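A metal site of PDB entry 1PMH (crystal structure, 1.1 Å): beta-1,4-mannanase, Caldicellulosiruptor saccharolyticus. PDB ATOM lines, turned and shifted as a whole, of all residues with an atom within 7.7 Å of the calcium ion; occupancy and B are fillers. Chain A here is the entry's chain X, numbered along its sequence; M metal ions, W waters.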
ATOM      1  N   LEU A   9      -9.534   5.292  30.451  1.00  0.00           N
ATOM      2  CA  LEU A   9      -8.556   5.265  29.367  1.00  0.00           C
ATOM      3  C   LEU A   9      -9.191   4.486  28.212  1.00  0.00           C
ATOM      4  O   LEU A   9      -9.011   3.281  28.028  1.00  0.00           O
ATOM      5  CB  LEU A   9      -7.254   4.657  29.873  1.00  0.00           C
ATOM      6  CG  LEU A   9      -6.717   5.195  31.193  1.00  0.00           C
ATOM      7  CD1 LEU A   9      -5.370   4.597  31.527  1.00  0.00           C
ATOM      8  CD2 LEU A   9      -6.570   6.719  31.133  1.00  0.00           C
ATOM      9  N   ASP A  10      -9.951   5.244  27.429  1.00  0.00           N
ATOM     10  CA  ASP A  10     -10.764   4.725  26.342  1.00  0.00           C
ATOM     11  C   ASP A  10     -10.238   5.070  24.944  1.00  0.00           C
ATOM     12  O   ASP A  10     -10.830   4.660  23.954  1.00  0.00           O
ATOM     13  CB  ASP A  10     -12.237   5.128  26.451  1.00  0.00           C
ATOM     14  CG  ASP A  10     -12.454   6.614  26.446  1.00  0.00           C
ATOM     15  OD1 ASP A  10     -11.515   7.393  26.194  1.00  0.00           O
ATOM     16  OD2 ASP A  10     -13.618   7.029  26.696  1.00  0.00           O
ATOM     17  N   PHE A  11      -9.163   5.842  24.891  1.00  0.00           N
ATOM     18  CA  PHE A  11      -8.480   6.261  23.684  1.00  0.00           C
ATOM     19  C   PHE A  11      -9.360   7.162  22.812  1.00  0.00           C
ATOM     20  O   PHE A  11      -9.007   7.415  21.662  1.00  0.00           O
ATOM     21  CB  PHE A  11      -7.886   5.061  22.927  1.00  0.00           C
ATOM     22  CG  PHE A  11      -7.079   4.212  23.866  1.00  0.00           C
ATOM     23  CD1 PHE A  11      -5.821   4.641  24.273  1.00  0.00           C
ATOM     24  CD2 PHE A  11      -7.621   3.075  24.452  1.00  0.00           C
ATOM     25  CE1 PHE A  11      -5.105   3.955  25.231  1.00  0.00           C
ATOM     26  CE2 PHE A  11      -6.906   2.367  25.445  1.00  0.00           C
ATOM     27  CZ  PHE A  11      -5.665   2.799  25.805  1.00  0.00           C
ATOM     28  N   GLU A  12     -10.477   7.671  23.325  1.00  0.00           N
ATOM     29  CA  GLU A  12     -11.451   8.321  22.482  1.00  0.00           C
ATOM     30  C   GLU A  12     -11.017   9.727  22.066  1.00  0.00           C
ATOM     31  O   GLU A  12     -11.610  10.283  21.157  1.00  0.00           O
ATOM     32  CB  GLU A  12     -12.844   8.273  23.099  1.00  0.00           C
ATOM     33  CG  GLU A  12     -13.434   6.866  23.098  1.00  0.00           C
ATOM     34  CD  GLU A  12     -13.461   6.241  21.716  1.00  0.00           C
ATOM     35  OE1 GLU A  12     -14.177   6.743  20.783  1.00  0.00           O
ATOM     36  OE2 GLU A  12     -12.747   5.216  21.547  1.00  0.00           O
ATOM     37  N   ASP A  13      -9.971  10.254  22.675  1.00  0.00           N
ATOM     38  CA  ASP A  13      -9.292  11.460  22.169  1.00  0.00           C
ATOM     39  C   ASP A  13      -8.374  11.255  20.971  1.00  0.00           C
ATOM     40  O   ASP A  13      -7.707  12.197  20.500  1.00  0.00           O
ATOM     41  CB  ASP A  13      -8.603  12.230  23.296  1.00  0.00           C
ATOM     42  CG  ASP A  13      -7.395  11.519  23.865  1.00  0.00           C
ATOM     43  OD1 ASP A  13      -7.031  10.409  23.412  1.00  0.00           O
ATOM     44  OD2 ASP A  13      -6.754  12.072  24.793  1.00  0.00           O
ATOM     45  N   VAL A  35      -2.463   4.199  18.176  1.00  0.00           N
ATOM     46  CA  VAL A  35      -3.906   4.333  18.303  1.00  0.00           C
ATOM     47  C   VAL A  35      -4.474   3.903  16.956  1.00  0.00           C
ATOM     48  O   VAL A  35      -3.973   4.277  15.920  1.00  0.00           O
ATOM     49  CB  VAL A  35      -4.312   5.733  18.834  1.00  0.00           C
ATOM     50  CG1 VAL A  35      -3.869   6.860  17.896  1.00  0.00           C
ATOM     51  CG2 VAL A  35      -5.782   5.774  19.174  1.00  0.00           C
ATOM     52  N   SER A  36      -5.550   3.144  17.006  1.00  0.00           N
ATOM     53  CA  SER A  36      -6.146   2.562  15.834  1.00  0.00           C
ATOM     54  C   SER A  36      -7.650   2.750  15.782  1.00  0.00           C
ATOM     55  O   SER A  36      -8.308   2.684  16.800  1.00  0.00           O
ATOM     56  CB  SER A  36      -5.796   1.066  15.835  1.00  0.00           C
ATOM     57  OG  SER A  36      -6.352   0.324  14.776  1.00  0.00           O
ATOM     58  N   LEU A  39     -11.154  -1.171  15.203  1.00  0.00           N
ATOM     59  CA  LEU A  39     -12.303  -1.662  15.944  1.00  0.00           C
ATOM     60  C   LEU A  39     -13.441  -0.619  15.966  1.00  0.00           C
ATOM     61  O   LEU A  39     -14.320  -0.727  16.799  1.00  0.00           O
ATOM     62  CB  LEU A  39     -11.924  -2.135  17.342  1.00  0.00           C
ATOM     63  CG  LEU A  39     -10.743  -3.110  17.411  1.00  0.00           C
ATOM     64  CD1 LEU A  39     -10.487  -3.496  18.828  1.00  0.00           C
ATOM     65  CD2 LEU A  39     -10.958  -4.334  16.583  1.00  0.00           C
ATOM     66  N   ARG A  41     -16.570   1.411  16.035  1.00  0.00           N
ATOM     67  CA  ARG A  41     -17.928   0.974  16.085  1.00  0.00           C
ATOM     68  C   ARG A  41     -18.764   1.997  16.845  1.00  0.00           C
ATOM     69  O   ARG A  41     -18.211   2.987  17.267  1.00  0.00           O
ATOM     70  CB  ARG A  41     -17.972  -0.413  16.636  1.00  0.00           C
ATOM     71  CG  ARG A  41     -17.469  -0.500  18.045  1.00  0.00           C
ATOM     72  CD  ARG A  41     -17.170  -1.981  18.386  1.00  0.00           C
ATOM     73  NE  ARG A  41     -16.731  -2.247  19.739  1.00  0.00           N
ATOM     74  CZ  ARG A  41     -15.489  -2.145  20.186  1.00  0.00           C
ATOM     75  NH1 ARG A  41     -14.577  -1.650  19.374  1.00  0.00           N
ATOM     76  NH2 ARG A  41     -15.173  -2.420  21.461  1.00  0.00           N
ATOM     77  N   GLY A  43     -20.089   4.610  19.060  1.00  0.00           N
ATOM     78  CA  GLY A  43     -19.661   5.181  20.317  1.00  0.00           C
ATOM     79  C   GLY A  43     -18.265   4.769  20.747  1.00  0.00           C
ATOM     80  O   GLY A  43     -17.890   5.048  21.865  1.00  0.00           O
ATOM     81  N   ASN A  44     -17.468   4.165  19.863  1.00  0.00           N
ATOM     82  CA  ASN A  44     -16.160   3.678  20.256  1.00  0.00           C
ATOM     83  C   ASN A  44     -15.267   3.623  19.022  1.00  0.00           C
ATOM     84  O   ASN A  44     -15.219   2.653  18.299  1.00  0.00           O
ATOM     85  CB  ASN A  44     -16.272   2.304  20.862  1.00  0.00           C
ATOM     86  CG  ASN A  44     -14.935   1.857  21.446  1.00  0.00           C
ATOM     87  OD1 ASN A  44     -13.914   2.521  21.229  1.00  0.00           O
ATOM     88  ND2 ASN A  44     -14.910   0.730  22.116  1.00  0.00           N
ATOM     89  N   LYS A  45     -14.613   4.749  18.786  1.00  0.00           N
ATOM     90  CA  LYS A  45     -13.872   4.961  17.543  1.00  0.00           C
ATOM     91  C   LYS A  45     -12.416   4.445  17.551  1.00  0.00           C
ATOM     92  O   LYS A  45     -11.908   4.004  16.518  1.00  0.00           O
ATOM     93  CB  LYS A  45     -13.817   6.442  17.205  1.00  0.00           C
ATOM     94  CG  LYS A  45     -13.168   6.808  15.881  1.00  0.00           C
ATOM     95  CD  LYS A  45     -13.548   8.245  15.606  1.00  0.00           C
ATOM     96  CE  LYS A  45     -13.044   8.780  14.316  1.00  0.00           C
ATOM     97  NZ  LYS A  45     -13.813  10.041  13.984  1.00  0.00           N
ATOM     98  N   TYR A  46     -11.785   4.478  18.730  1.00  0.00           N
ATOM     99  CA  TYR A  46     -10.368   4.214  18.839  1.00  0.00           C
ATOM    100  C   TYR A  46     -10.034   3.130  19.848  1.00  0.00           C
ATOM    101  O   TYR A  46     -10.685   3.001  20.873  1.00  0.00           O
ATOM    102  CB  TYR A  46      -9.596   5.481  19.263  1.00  0.00           C
ATOM    103  CG  TYR A  46      -9.708   6.677  18.328  1.00  0.00           C
ATOM    104  CD1 TYR A  46      -8.940   6.766  17.172  1.00  0.00           C
ATOM    105  CD2 TYR A  46     -10.585   7.719  18.613  1.00  0.00           C
ATOM    106  CE1 TYR A  46      -9.048   7.883  16.306  1.00  0.00           C
ATOM    107  CE2 TYR A  46     -10.686   8.838  17.783  1.00  0.00           C
ATOM    108  CZ  TYR A  46      -9.917   8.903  16.648  1.00  0.00           C
ATOM    109  OH  TYR A  46      -9.994   9.988  15.820  1.00  0.00           O
ATOM    110  N   ALA A  47      -8.929   2.429  19.617  1.00  0.00           N
ATOM    111  CA  ALA A  47      -8.377   1.449  20.541  1.00  0.00           C
ATOM    112  C   ALA A  47      -6.870   1.506  20.452  1.00  0.00           C
ATOM    113  O   ALA A  47      -6.310   2.011  19.488  1.00  0.00           O
ATOM    114  CB  ALA A  47      -8.892   0.064  20.223  1.00  0.00           C
ATOM    115  N   LEU A  48      -6.217   0.964  21.467  1.00  0.00           N
ATOM    116  CA  LEU A  48      -4.782   0.860  21.500  1.00  0.00           C
ATOM    117  C   LEU A  48      -4.367  -0.404  20.795  1.00  0.00           C
ATOM    118  O   LEU A  48      -4.700  -1.490  21.227  1.00  0.00           O
ATOM    119  CB  LEU A  48      -4.267   0.917  22.929  1.00  0.00           C
ATOM    120  CG  LEU A  48      -2.749   1.114  23.096  1.00  0.00           C
ATOM    121  CD1 LEU A  48      -2.361   2.535  22.736  1.00  0.00           C
ATOM    122  CD2 LEU A  48      -2.332   0.745  24.490  1.00  0.00           C
ATOM    123  N   LEU A 175      -6.035  -3.161  23.171  1.00  0.00           N
ATOM    124  CA  LEU A 175      -6.583  -2.832  24.464  1.00  0.00           C
ATOM    125  C   LEU A 175      -7.565  -1.683  24.306  1.00  0.00           C
ATOM    126  O   LEU A 175      -7.355  -0.755  23.524  1.00  0.00           O
ATOM    127  CB  LEU A 175      -5.537  -2.419  25.462  1.00  0.00           C
ATOM    128  CG  LEU A 175      -4.615  -3.474  25.963  1.00  0.00           C
ATOM    129  CD1 LEU A 175      -3.558  -2.833  26.869  1.00  0.00           C
ATOM    130  CD2 LEU A 175      -5.367  -4.540  26.758  1.00  0.00           C
ATOM    131  N   ASP A 176      -8.630  -1.719  25.089  1.00  0.00           N
ATOM    132  CA  ASP A 176      -9.559  -0.578  25.128  1.00  0.00           C
ATOM    133  C   ASP A 176     -10.217  -0.561  26.506  1.00  0.00           C
ATOM    134  O   ASP A 176     -10.227  -1.542  27.257  1.00  0.00           O
ATOM    135  CB  ASP A 176     -10.602  -0.675  24.011  1.00  0.00           C
ATOM    136  CG  ASP A 176     -11.196   0.651  23.568  1.00  0.00           C
ATOM    137  OD1 ASP A 176     -10.868   1.700  24.156  1.00  0.00           O
ATOM    138  OD2 ASP A 176     -12.006   0.665  22.643  1.00  0.00           O
ATOM    139  N   ASN A 177     -10.834   0.592  26.782  1.00  0.00           N
ATOM    140  CA  ASN A 177     -11.663   0.731  27.975  1.00  0.00           C
ATOM    141  C   ASN A 177     -10.948   0.252  29.231  1.00  0.00           C
ATOM    142  O   ASN A 177     -11.494  -0.513  30.042  1.00  0.00           O
ATOM    143  CB  ASN A 177     -12.997   0.033  27.764  1.00  0.00           C
ATOM    144  CG  ASN A 177     -13.800   0.708  26.667  1.00  0.00           C
ATOM    145  OD1 ASN A 177     -13.685   1.920  26.467  1.00  0.00           O
ATOM    146  ND2 ASN A 177     -14.599  -0.042  25.967  1.00  0.00           N
ATOM    147  N   VAL A 178      -9.738   0.764  29.381  1.00  0.00           N
ATOM    148  CA  VAL A 178      -8.997   0.502  30.622  1.00  0.00           C
ATOM    149  C   VAL A 178      -9.510   1.520  31.631  1.00  0.00           C
ATOM    150  O   VAL A 178      -9.399   2.697  31.409  1.00  0.00           O
ATOM    151  CB  VAL A 178      -7.486   0.652  30.368  1.00  0.00           C
ATOM    152  CG1 VAL A 178      -6.737   0.519  31.691  1.00  0.00           C
ATOM    153  CG2 VAL A 178      -7.018  -0.386  29.322  1.00  0.00           C
HETATM  154 CA    CA M   1     -12.128   3.215  22.628  1.00  0.00          CA
HETATM  155  O   HOH W   1     -13.876   3.273  24.149  1.00  0.00           O
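The side-chain carboxylate of Glu 12 sits at hydrogen-bond distance from the backbone NH of Lys 45 (2.9 Å).
The side-chain amide nitrogen of Asn 44 lies close to the guanidinium group of Arg 41.
The nearest printed residue that does not touch the calcium ion is Asn 177 (4.3 Å).
The calcium ion is bound by the backbone carbonyl oxygen (O) of Tyr 46 (2.3 Å), water W1 (2.3 Å), the backbone carbonyl oxygen (O) of Asp 10 (2.4 Å), the side-chain carboxylate (OE2) of Glu 12 (2.4 Å), the side-chain amide oxygen (OD1) of Asn 44 (2.4 Å), the side-chain carboxylate (OD1) of Asp 176 (2.5 Å) and the side-chain carboxylate (OD2) of Asp 176 (2.6 Å).
Water W1 lies within hydrogen-bond range of OD1 of Asn 177 and ND2 of Asn 44.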
